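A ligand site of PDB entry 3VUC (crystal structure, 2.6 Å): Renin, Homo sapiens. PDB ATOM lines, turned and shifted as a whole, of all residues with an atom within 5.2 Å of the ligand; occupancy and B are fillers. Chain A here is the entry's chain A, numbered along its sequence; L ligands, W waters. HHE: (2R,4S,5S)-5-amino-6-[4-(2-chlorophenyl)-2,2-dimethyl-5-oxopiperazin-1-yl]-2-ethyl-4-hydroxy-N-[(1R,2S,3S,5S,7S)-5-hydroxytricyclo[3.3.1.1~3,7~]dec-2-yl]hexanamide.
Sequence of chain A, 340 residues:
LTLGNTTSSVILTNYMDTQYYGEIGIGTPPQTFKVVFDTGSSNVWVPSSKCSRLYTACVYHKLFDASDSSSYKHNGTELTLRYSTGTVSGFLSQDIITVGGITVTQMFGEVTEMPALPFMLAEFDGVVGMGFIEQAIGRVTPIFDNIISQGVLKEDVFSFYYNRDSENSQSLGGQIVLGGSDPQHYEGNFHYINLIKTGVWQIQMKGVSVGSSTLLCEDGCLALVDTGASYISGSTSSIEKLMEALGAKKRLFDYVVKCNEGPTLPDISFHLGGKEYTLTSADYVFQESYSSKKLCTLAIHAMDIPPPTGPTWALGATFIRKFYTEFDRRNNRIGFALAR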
ATOM      1  N   THR A  18       2.850  -1.456  -4.617  1.00  0.00           N
ATOM      2  CA  THR A  18       1.563  -1.162  -5.180  1.00  0.00           C
ATOM      3  C   THR A  18       0.429  -1.967  -4.528  1.00  0.00           C
ATOM      4  O   THR A  18      -0.724  -1.570  -4.643  1.00  0.00           O
ATOM      5  CB  THR A  18       1.488  -1.329  -6.712  1.00  0.00           C
ATOM      6  OG1 THR A  18       1.903  -2.643  -7.055  1.00  0.00           O
ATOM      7  CG2 THR A  18       2.359  -0.361  -7.444  1.00  0.00           C
ATOM      8  N   GLN A  19       0.751  -3.077  -3.899  1.00  0.00           N
ATOM      9  CA  GLN A  19      -0.290  -3.922  -3.343  1.00  0.00           C
ATOM     10  C   GLN A  19       0.272  -4.383  -2.025  1.00  0.00           C
ATOM     11  O   GLN A  19       1.426  -4.902  -1.996  1.00  0.00           O
ATOM     12  CB  GLN A  19      -0.588  -5.142  -4.244  1.00  0.00           C
ATOM     13  CG  GLN A  19      -1.007  -4.801  -5.662  1.00  0.00           C
ATOM     14  CD  GLN A  19      -1.049  -5.999  -6.620  1.00  0.00           C
ATOM     15  OE1 GLN A  19      -1.485  -7.093  -6.272  1.00  0.00           O
ATOM     16  NE2 GLN A  19      -0.612  -5.786  -7.819  1.00  0.00           N
ATOM     17  N   VAL A  36      -6.295  -7.767   0.396  1.00  0.00           N
ATOM     18  CA  VAL A  36      -5.997  -6.350   0.582  1.00  0.00           C
ATOM     19  C   VAL A  36      -7.023  -5.823   1.567  1.00  0.00           C
ATOM     20  O   VAL A  36      -8.234  -6.147   1.466  1.00  0.00           O
ATOM     21  CB  VAL A  36      -6.167  -5.600  -0.726  1.00  0.00           C
ATOM     22  CG1 VAL A  36      -6.021  -4.121  -0.482  1.00  0.00           C
ATOM     23  CG2 VAL A  36      -5.111  -6.041  -1.744  1.00  0.00           C
ATOM     24  N   ASP A  38      -8.963  -2.861   2.511  1.00  0.00           N
ATOM     25  CA  ASP A  38      -9.343  -1.793   1.580  1.00  0.00           C
ATOM     26  C   ASP A  38     -10.366  -0.813   2.209  1.00  0.00           C
ATOM     27  O   ASP A  38     -11.558  -1.122   2.225  1.00  0.00           O
ATOM     28  CB  ASP A  38      -9.939  -2.414   0.288  1.00  0.00           C
ATOM     29  CG  ASP A  38     -10.490  -1.368  -0.657  1.00  0.00           C
ATOM     30  OD1 ASP A  38      -9.882  -0.289  -0.707  1.00  0.00           O
ATOM     31  OD2 ASP A  38     -11.534  -1.595  -1.350  1.00  0.00           O
ATOM     32  N   GLY A  40     -11.509   1.739   1.008  1.00  0.00           N
ATOM     33  CA  GLY A  40     -12.369   2.357   0.020  1.00  0.00           C
ATOM     34  C   GLY A  40     -13.688   1.613  -0.186  1.00  0.00           C
ATOM     35  O   GLY A  40     -14.538   2.089  -0.928  1.00  0.00           O
ATOM     36  N   SER A  41     -13.840   0.435   0.437  1.00  0.00           N
ATOM     37  CA  SER A  41     -14.984  -0.431   0.175  1.00  0.00           C
ATOM     38  C   SER A  41     -15.323  -1.171   1.475  1.00  0.00           C
ATOM     39  O   SER A  41     -14.543  -1.061   2.431  1.00  0.00           O
ATOM     40  CB  SER A  41     -14.697  -1.389  -1.005  1.00  0.00           C
ATOM     41  OG  SER A  41     -13.847  -2.479  -0.654  1.00  0.00           O
ATOM     42  N   SER A  42     -16.449  -1.903   1.554  1.00  0.00           N
ATOM     43  CA  SER A  42     -16.877  -2.536   2.844  1.00  0.00           C
ATOM     44  C   SER A  42     -17.283  -4.010   2.792  1.00  0.00           C
ATOM     45  O   SER A  42     -17.755  -4.559   3.792  1.00  0.00           O
ATOM     46  CB  SER A  42     -17.997  -1.758   3.491  1.00  0.00           C
ATOM     47  OG  SER A  42     -17.745  -0.368   3.328  1.00  0.00           O
ATOM     48  N   TRP A  45     -14.588 -10.232  -0.054  1.00  0.00           N
ATOM     49  CA  TRP A  45     -14.763 -11.322  -1.036  1.00  0.00           C
ATOM     50  C   TRP A  45     -13.492 -12.006  -1.440  1.00  0.00           C
ATOM     51  O   TRP A  45     -12.423 -11.417  -1.439  1.00  0.00           O
ATOM     52  CB  TRP A  45     -15.383 -10.802  -2.291  1.00  0.00           C
ATOM     53  CG  TRP A  45     -14.524  -9.787  -3.011  1.00  0.00           C
ATOM     54  CD1 TRP A  45     -14.585  -8.446  -2.889  1.00  0.00           C
ATOM     55  CD2 TRP A  45     -13.492 -10.047  -3.981  1.00  0.00           C
ATOM     56  NE1 TRP A  45     -13.666  -7.841  -3.717  1.00  0.00           N
ATOM     57  CE2 TRP A  45     -12.984  -8.816  -4.390  1.00  0.00           C
ATOM     58  CE3 TRP A  45     -12.975 -11.204  -4.545  1.00  0.00           C
ATOM     59  CZ2 TRP A  45     -11.975  -8.697  -5.342  1.00  0.00           C
ATOM     60  CZ3 TRP A  45     -11.972 -11.089  -5.489  1.00  0.00           C
ATOM     61  CH2 TRP A  45     -11.495  -9.841  -5.885  1.00  0.00           C
ATOM     62  N   LEU A  81     -19.740  -5.720  -7.196  1.00  0.00           N
ATOM     63  CA  LEU A  81     -18.922  -4.673  -6.622  1.00  0.00           C
ATOM     64  C   LEU A  81     -18.256  -4.034  -7.802  1.00  0.00           C
ATOM     65  O   LEU A  81     -17.558  -4.704  -8.600  1.00  0.00           O
ATOM     66  CB  LEU A  81     -17.893  -5.265  -5.682  1.00  0.00           C
ATOM     67  CG  LEU A  81     -18.501  -6.011  -4.511  1.00  0.00           C
ATOM     68  CD1 LEU A  81     -17.465  -6.938  -3.930  1.00  0.00           C
ATOM     69  CD2 LEU A  81     -18.924  -4.987  -3.461  1.00  0.00           C
ATOM     70  N   ARG A  82     -18.516  -2.723  -7.913  1.00  0.00           N
ATOM     71  CA  ARG A  82     -18.173  -1.945  -9.083  1.00  0.00           C
ATOM     72  C   ARG A  82     -17.325  -0.862  -8.563  1.00  0.00           C
ATOM     73  O   ARG A  82     -17.829   0.228  -8.305  1.00  0.00           O
ATOM     74  CB  ARG A  82     -19.402  -1.294  -9.760  1.00  0.00           C
ATOM     75  CG  ARG A  82     -20.190  -2.209 -10.683  1.00  0.00           C
ATOM     76  CD  ARG A  82     -21.442  -1.527 -11.163  1.00  0.00           C
ATOM     77  NE  ARG A  82     -22.477  -2.457 -11.645  1.00  0.00           N
ATOM     78  CZ  ARG A  82     -23.407  -3.050 -10.868  1.00  0.00           C
ATOM     79  NH1 ARG A  82     -23.430  -2.835  -9.537  1.00  0.00           N
ATOM     80  NH2 ARG A  82     -24.315  -3.858 -11.421  1.00  0.00           N
ATOM     81  N   TYR A  83     -16.049  -1.176  -8.401  1.00  0.00           N
ATOM     82  CA  TYR A  83     -15.015  -0.231  -7.999  1.00  0.00           C
ATOM     83  C   TYR A  83     -14.733   0.662  -9.171  1.00  0.00           C
ATOM     84  O   TYR A  83     -15.061   0.332 -10.303  1.00  0.00           O
ATOM     85  CB  TYR A  83     -13.731  -0.981  -7.665  1.00  0.00           C
ATOM     86  CG  TYR A  83     -13.850  -2.080  -6.666  1.00  0.00           C
ATOM     87  CD1 TYR A  83     -13.435  -3.393  -6.972  1.00  0.00           C
ATOM     88  CD2 TYR A  83     -14.379  -1.830  -5.381  1.00  0.00           C
ATOM     89  CE1 TYR A  83     -13.533  -4.417  -6.003  1.00  0.00           C
ATOM     90  CE2 TYR A  83     -14.499  -2.860  -4.428  1.00  0.00           C
ATOM     91  CZ  TYR A  83     -14.089  -4.110  -4.748  1.00  0.00           C
ATOM     92  OH  TYR A  83     -14.179  -5.057  -3.767  1.00  0.00           O
ATOM     93  N   SER A  84     -14.088   1.794  -8.904  1.00  0.00           N
ATOM     94  CA  SER A  84     -13.670   2.703  -9.974  1.00  0.00           C
ATOM     95  C   SER A  84     -12.734   2.088 -11.001  1.00  0.00           C
ATOM     96  O   SER A  84     -12.676   2.572 -12.106  1.00  0.00           O
ATOM     97  CB  SER A  84     -13.018   3.966  -9.412  1.00  0.00           C
ATOM     98  OG  SER A  84     -11.762   3.673  -8.793  1.00  0.00           O
ATOM     99  N   THR A  85     -12.030   1.026 -10.641  1.00  0.00           N
ATOM    100  CA  THR A  85     -11.034   0.483 -11.564  1.00  0.00           C
ATOM    101  C   THR A  85     -11.375  -0.920 -12.069  1.00  0.00           C
ATOM    102  O   THR A  85     -10.556  -1.518 -12.763  1.00  0.00           O
ATOM    103  CB  THR A  85      -9.590   0.412 -10.937  1.00  0.00           C
ATOM    104  OG1 THR A  85      -9.674  -0.235  -9.667  1.00  0.00           O
ATOM    105  CG2 THR A  85      -8.975   1.773 -10.767  1.00  0.00           C
ATOM    106  N   PRO A 118      -8.591  -5.908 -14.210  1.00  0.00           N
ATOM    107  CA  PRO A 118      -7.269  -5.881 -13.617  1.00  0.00           C
ATOM    108  C   PRO A 118      -6.839  -7.166 -12.945  1.00  0.00           C
ATOM    109  O   PRO A 118      -5.671  -7.257 -12.594  1.00  0.00           O
ATOM    110  CB  PRO A 118      -7.433  -4.858 -12.497  1.00  0.00           C
ATOM    111  CG  PRO A 118      -8.824  -5.076 -12.018  1.00  0.00           C
ATOM    112  CD  PRO A 118      -9.589  -5.258 -13.331  1.00  0.00           C
ATOM    113  N   PHE A 119      -7.729  -8.134 -12.734  1.00  0.00           N
ATOM    114  CA  PHE A 119      -7.384  -9.139 -11.724  1.00  0.00           C
ATOM    115  C   PHE A 119      -6.168 -10.024 -11.984  1.00  0.00           C
ATOM    116  O   PHE A 119      -5.515 -10.482 -11.032  1.00  0.00           O
ATOM    117  CB  PHE A 119      -8.637  -9.810 -11.089  1.00  0.00           C
ATOM    118  CG  PHE A 119      -9.572  -8.784 -10.412  1.00  0.00           C
ATOM    119  CD1 PHE A 119      -9.296  -8.281  -9.165  1.00  0.00           C
ATOM    120  CD2 PHE A 119     -10.665  -8.266 -11.087  1.00  0.00           C
ATOM    121  CE1 PHE A 119     -10.106  -7.293  -8.565  1.00  0.00           C
ATOM    122  CE2 PHE A 119     -11.492  -7.285 -10.487  1.00  0.00           C
ATOM    123  CZ  PHE A 119     -11.199  -6.809  -9.228  1.00  0.00           C
ATOM    124  N   LEU A 121      -3.484  -8.944 -12.821  1.00  0.00           N
ATOM    125  CA  LEU A 121      -2.346  -8.210 -12.319  1.00  0.00           C
ATOM    126  C   LEU A 121      -2.357  -8.142 -10.794  1.00  0.00           C
ATOM    127  O   LEU A 121      -1.505  -7.466 -10.217  1.00  0.00           O
ATOM    128  CB  LEU A 121      -2.284  -6.792 -12.884  1.00  0.00           C
ATOM    129  CG  LEU A 121      -2.240  -6.551 -14.398  1.00  0.00           C
ATOM    130  CD1 LEU A 121      -2.314  -5.044 -14.612  1.00  0.00           C
ATOM    131  CD2 LEU A 121      -1.011  -7.106 -15.085  1.00  0.00           C
ATOM    132  N   ALA A 122      -3.282  -8.848 -10.135  1.00  0.00           N
ATOM    133  CA  ALA A 122      -3.311  -8.881  -8.675  1.00  0.00           C
ATOM    134  C   ALA A 122      -2.470 -10.030  -8.155  1.00  0.00           C
ATOM    135  O   ALA A 122      -2.658 -11.197  -8.556  1.00  0.00           O
ATOM    136  CB  ALA A 122      -4.725  -9.037  -8.160  1.00  0.00           C
ATOM    137  N   PHE A 124      -2.722 -10.417  -4.903  1.00  0.00           N
ATOM    138  CA  PHE A 124      -3.651 -10.862  -3.853  1.00  0.00           C
ATOM    139  C   PHE A 124      -4.776 -11.699  -4.476  1.00  0.00           C
ATOM    140  O   PHE A 124      -4.966 -11.641  -5.723  1.00  0.00           O
ATOM    141  CB  PHE A 124      -4.243  -9.651  -3.151  1.00  0.00           C
ATOM    142  CG  PHE A 124      -4.998  -8.684  -4.079  1.00  0.00           C
ATOM    143  CD1 PHE A 124      -4.344  -7.582  -4.651  1.00  0.00           C
ATOM    144  CD2 PHE A 124      -6.344  -8.877  -4.371  1.00  0.00           C
ATOM    145  CE1 PHE A 124      -5.041  -6.704  -5.519  1.00  0.00           C
ATOM    146  CE2 PHE A 124      -7.038  -8.008  -5.228  1.00  0.00           C
ATOM    147  CZ  PHE A 124      -6.386  -6.901  -5.786  1.00  0.00           C
ATOM    148  N   VAL A 127     -10.367  -9.263  -1.329  1.00  0.00           N
ATOM    149  CA  VAL A 127     -10.419  -7.978  -0.690  1.00  0.00           C
ATOM    150  C   VAL A 127     -11.127  -8.090   0.659  1.00  0.00           C
ATOM    151  O   VAL A 127     -12.119  -8.820   0.783  1.00  0.00           O
ATOM    152  CB  VAL A 127     -11.170  -7.007  -1.589  1.00  0.00           C
ATOM    153  CG1 VAL A 127     -11.494  -5.656  -0.864  1.00  0.00           C
ATOM    154  CG2 VAL A 127     -10.365  -6.792  -2.885  1.00  0.00           C
ATOM    155  N   GLN A 135     -21.665   1.688   3.136  1.00  0.00           N
ATOM    156  CA  GLN A 135     -21.225   1.527   1.771  1.00  0.00           C
ATOM    157  C   GLN A 135     -21.146   0.057   1.395  1.00  0.00           C
ATOM    158  O   GLN A 135     -20.719  -0.268   0.302  1.00  0.00           O
ATOM    159  CB  GLN A 135     -19.915   2.310   1.503  1.00  0.00           C
ATOM    160  CG  GLN A 135     -20.127   3.788   1.131  1.00  0.00           C
ATOM    161  CD  GLN A 135     -18.785   4.418   0.807  1.00  0.00           C
ATOM    162  OE1 GLN A 135     -18.618   5.172  -0.182  1.00  0.00           O
ATOM    163  NE2 GLN A 135     -17.790   4.080   1.633  1.00  0.00           N
ATOM    164  N   ILE A 137     -22.274  -3.374   0.015  1.00  0.00           N
ATOM    165  CA  ILE A 137     -23.274  -3.767  -0.970  1.00  0.00           C
ATOM    166  C   ILE A 137     -23.986  -4.931  -0.347  1.00  0.00           C
ATOM    167  O   ILE A 137     -23.351  -5.691   0.346  1.00  0.00           O
ATOM    168  CB  ILE A 137     -22.647  -4.151  -2.362  1.00  0.00           C
ATOM    169  CG1 ILE A 137     -21.911  -2.970  -2.989  1.00  0.00           C
ATOM    170  CG2 ILE A 137     -23.719  -4.601  -3.352  1.00  0.00           C
ATOM    171  CD1 ILE A 137     -22.832  -1.802  -3.239  1.00  0.00           C
ATOM    172  N   LEU A 224     -10.447  11.108  -0.216  1.00  0.00           N
ATOM    173  CA  LEU A 224     -10.748   9.766   0.211  1.00  0.00           C
ATOM    174  C   LEU A 224      -9.430   9.125   0.685  1.00  0.00           C
ATOM    175  O   LEU A 224      -8.394   9.235  -0.004  1.00  0.00           O
ATOM    176  CB  LEU A 224     -11.361   8.992  -0.956  1.00  0.00           C
ATOM    177  CG  LEU A 224     -11.708   7.561  -0.595  1.00  0.00           C
ATOM    178  CD1 LEU A 224     -12.919   7.458   0.364  1.00  0.00           C
ATOM    179  CD2 LEU A 224     -11.917   6.744  -1.832  1.00  0.00           C
ATOM    180  N   ASP A 226      -7.610   5.860   1.071  1.00  0.00           N
ATOM    181  CA  ASP A 226      -7.925   4.552   0.522  1.00  0.00           C
ATOM    182  C   ASP A 226      -6.731   3.613   0.623  1.00  0.00           C
ATOM    183  O   ASP A 226      -5.804   3.653  -0.200  1.00  0.00           O
ATOM    184  CB  ASP A 226      -8.402   4.719  -0.942  1.00  0.00           C
ATOM    185  CG  ASP A 226      -8.804   3.397  -1.587  1.00  0.00           C
ATOM    186  OD1 ASP A 226      -8.735   2.371  -0.891  1.00  0.00           O
ATOM    187  OD2 ASP A 226      -9.216   3.391  -2.773  1.00  0.00           O
ATOM    188  N   GLY A 228      -6.528   0.651  -0.013  1.00  0.00           N
ATOM    189  CA  GLY A 228      -6.495  -0.320  -1.092  1.00  0.00           C
ATOM    190  C   GLY A 228      -6.183   0.278  -2.468  1.00  0.00           C
ATOM    191  O   GLY A 228      -6.388  -0.384  -3.464  1.00  0.00           O
ATOM    192  N   ALA A 229      -5.701   1.514  -2.505  1.00  0.00           N
ATOM    193  CA  ALA A 229      -5.317   2.199  -3.751  1.00  0.00           C
ATOM    194  C   ALA A 229      -3.799   2.307  -3.725  1.00  0.00           C
ATOM    195  O   ALA A 229      -3.189   2.610  -2.668  1.00  0.00           O
ATOM    196  CB  ALA A 229      -5.923   3.595  -3.813  1.00  0.00           C
ATOM    197  N   SER A 230      -3.194   2.053  -4.879  1.00  0.00           N
ATOM    198  CA  SER A 230      -1.778   2.020  -4.998  1.00  0.00           C
ATOM    199  C   SER A 230      -1.267   3.412  -4.829  1.00  0.00           C
ATOM    200  O   SER A 230      -0.218   3.625  -4.213  1.00  0.00           O
ATOM    201  CB  SER A 230      -1.346   1.502  -6.355  1.00  0.00           C
ATOM    202  OG  SER A 230      -1.590   0.121  -6.456  1.00  0.00           O
ATOM    203  N   ILE A 305     -13.335   9.298  -9.749  1.00  0.00           N
ATOM    204  CA  ILE A 305     -14.162   8.512  -8.878  1.00  0.00           C
ATOM    205  C   ILE A 305     -15.630   8.997  -9.024  1.00  0.00           C
ATOM    206  O   ILE A 305     -15.926  10.204  -8.901  1.00  0.00           O
ATOM    207  CB  ILE A 305     -13.640   8.589  -7.447  1.00  0.00           C
ATOM    208  CG1 ILE A 305     -12.282   7.903  -7.389  1.00  0.00           C
ATOM    209  CG2 ILE A 305     -14.568   7.890  -6.550  1.00  0.00           C
ATOM    210  CD1 ILE A 305     -11.450   8.187  -6.155  1.00  0.00           C
ATOM    211  N   THR A 309     -19.433   9.283  -4.040  1.00  0.00           N
ATOM    212  CA  THR A 309     -18.161   9.442  -3.347  1.00  0.00           C
ATOM    213  C   THR A 309     -17.251  10.455  -4.075  1.00  0.00           C
ATOM    214  O   THR A 309     -16.584  11.263  -3.431  1.00  0.00           O
ATOM    215  CB  THR A 309     -17.471   8.104  -3.136  1.00  0.00           C
ATOM    216  OG1 THR A 309     -18.404   7.188  -2.519  1.00  0.00           O
ATOM    217  CG2 THR A 309     -16.228   8.260  -2.288  1.00  0.00           C
HETATM  218  C1  HHE L   1     -16.819   1.317  -4.540  1.00  0.00           C
HETATM  219  C2  HHE L   1     -17.392   0.296  -3.550  1.00  0.00           C
HETATM  220  C3  HHE L   1     -17.832   2.450  -4.662  1.00  0.00           C
HETATM  221  C4  HHE L   1     -18.682  -0.296  -4.134  1.00  0.00           C
HETATM  222  C5  HHE L   1     -19.133   1.921  -5.277  1.00  0.00           C
HETATM  223  C6  HHE L   1     -19.721   0.839  -4.358  1.00  0.00           C
HETATM  224  C7  HHE L   1     -18.141   3.088  -3.256  1.00  0.00           C
HETATM  225  C8  HHE L   1     -18.796   2.052  -2.308  1.00  0.00           C
HETATM  226  C9  HHE L   1     -17.761   0.930  -2.157  1.00  0.00           C
HETATM  227  C10 HHE L   1     -20.067   1.461  -2.981  1.00  0.00           C
HETATM  228  O11 HHE L   1     -20.849   0.310  -5.079  1.00  0.00           O
HETATM  229  N12 HHE L   1     -15.603   1.911  -3.951  1.00  0.00           N
HETATM  230  C13 HHE L   1     -11.975   0.837  -4.137  1.00  0.00           C
HETATM  231  C14 HHE L   1     -10.589   0.290  -4.514  1.00  0.00           C
HETATM  232  C15 HHE L   1     -10.468  -1.242  -4.481  1.00  0.00           C
HETATM  233  N16 HHE L   1      -9.625   0.881  -3.556  1.00  0.00           N
HETATM  234  N17 HHE L   1      -9.232  -1.703  -5.161  1.00  0.00           N
HETATM  235  C18 HHE L   1      -9.352  -1.534  -6.618  1.00  0.00           C
HETATM  236  C19 HHE L   1      -8.140  -2.046  -7.360  1.00  0.00           C
HETATM  237  N20 HHE L   1      -7.238  -2.894  -6.815  1.00  0.00           N
HETATM  238  C21 HHE L   1      -7.358  -3.378  -5.424  1.00  0.00           C
HETATM  239  C22 HHE L   1      -8.762  -3.114  -4.840  1.00  0.00           C
HETATM  240  C23 HHE L   1      -8.617  -3.331  -3.326  1.00  0.00           C
HETATM  241  C24 HHE L   1      -9.725  -4.186  -5.400  1.00  0.00           C
HETATM  242  C25 HHE L   1      -6.130  -3.326  -7.537  1.00  0.00           C
HETATM  243  C26 HHE L   1      -4.923  -2.695  -7.284  1.00  0.00           C
HETATM  244  C27 HHE L   1      -3.797  -3.140  -7.939  1.00  0.00           C
HETATM  245  C28 HHE L   1      -3.848  -4.164  -8.868  1.00  0.00           C
HETATM  246  C29 HHE L   1      -5.053  -4.800  -9.134  1.00  0.00           C
HETATM  247  C30 HHE L   1      -6.163  -4.364  -8.436  1.00  0.00           C
HETATM  248  O31 HHE L   1      -7.990  -1.691  -8.501  1.00  0.00           O
HETATM  249 CL   HHE L   1      -7.620  -5.136  -8.800  1.00  0.00          CL
HETATM  250  C33 HHE L   1     -12.017   2.338  -4.458  1.00  0.00           C
HETATM  251  C34 HHE L   1     -13.346   3.013  -4.080  1.00  0.00           C
HETATM  252  C35 HHE L   1     -14.591   2.398  -4.697  1.00  0.00           C
HETATM  253  O36 HHE L   1     -14.675   2.372  -5.902  1.00  0.00           O
HETATM  254  C37 HHE L   1     -13.276   4.510  -4.446  1.00  0.00           C
HETATM  255  O38 HHE L   1     -12.260   0.565  -2.734  1.00  0.00           O
HETATM  256  C39 HHE L   1     -14.581   5.237  -4.008  1.00  0.00           C
HETATM  257  O   HOH W   1     -21.189  -1.845  -6.629  1.00  0.00           O
HETATM  258  O   HOH W   2     -10.891   1.685  -7.548  1.00  0.00           O
HETATM  259  O   HOH W   3      -6.163  -1.545 -10.743  1.00  0.00           O
HETATM  260  O   HOH W   4     -15.642   4.303  -7.441  1.00  0.00           O
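NE2 of Gln 19 is in hydrogen-bond range of O of Leu 121, 3.1 Å away.
OD2 of Asp 38 sits at hydrogen-bond distance from OG of Ser 41, at 2.6 Å.
OH of Tyr 83 sits at hydrogen-bond distance from NE1 of Trp 45.
N of Gly 228 sits at hydrogen-bond distance from OD1 of Asp 226 (2.9 Å).
The backbone NH of Gly 40 is in hydrogen-bond range of the side-chain carboxylate of Asp 226, at 3.4 Å.
O of Val 127 is in hydrogen-bond range of N of Trp 45, 3.0 Å away.
The backbone NH (N) of Gly 40 sits close to the side-chain carboxylate (OD1) of Asp 38 (3.1 Å).
The side-chain amide oxygen (OE1) of Gln 135 sits at hydrogen-bond distance from the side-chain hydroxyl (OG1) of Thr 309, 3.1 Å away.
Merely in contact with the ligand: Gln 19 (3.8 Å), Val 36 (3.9 Å), Ser 41 (3.5 Å), Arg 82 (3.7 Å), Tyr 83 (3.4 Å), Pro 118 (3.4 Å), Phe 119 (3.3 Å), Phe 124 (3.7 Å), Val 127 (3.7 Å), Gln 135 (3.7 Å), Ile 137 (3.4 Å), Leu 224 (3.7 Å), Ile 305 (3.7 Å) and Thr 309 (3.8 Å).
20 residues have an atom within 4 Å of the ligand: Gln 19, Val 36, Asp 38, Gly 40, Ser 41, Arg 82, Tyr 83, Ser 84, Thr 85, Pro 118, Phe 119, Phe 124, Val 127, Gln 135, Ile 137, Leu 224, Asp 226, Gly 228, Ile 305 and Thr 309.
A nitrogen (N16) of the ligand lies within salt-bridge range of the side-chain carboxylate (OD1) of Asp 38 (3.1 Å).
A nitrogen (N12) of the ligand sits at hydrogen-bond distance from the backbone carbonyl oxygen (O) of Gly 40 (3.2 Å).
An oxygen (O36) of the ligand lies within hydrogen-bond range of the backbone NH (N) of Ser 84 (3.1 Å).
N16 of the ligand sits at hydrogen-bond distance from O of Gly 228 (3.5 Å).
A nitrogen (N16) of the ligand is in salt-bridge range of the side-chain carboxylate (OD2) of Asp 226.
The side-chain hydroxyl of Thr 85 lies within hydrogen-bond range of an oxygen (O31) of the ligand (2.5 Å).
Water W4 lies within hydrogen-bond range of an oxygen (O36) of the ligand (2.7 Å) and the backbone NH of Ser 84 (3.3 Å).
Water W1 lies within hydrogen-bond range of O11 of the ligand (2.7 Å) and N of Arg 82 (3.1 Å).
Water W2 lies within hydrogen-bond range of the side-chain hydroxyl (OG) of Ser 84 (2.5 Å) and the side-chain hydroxyl (OG1) of Thr 85 (3.1 Å).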
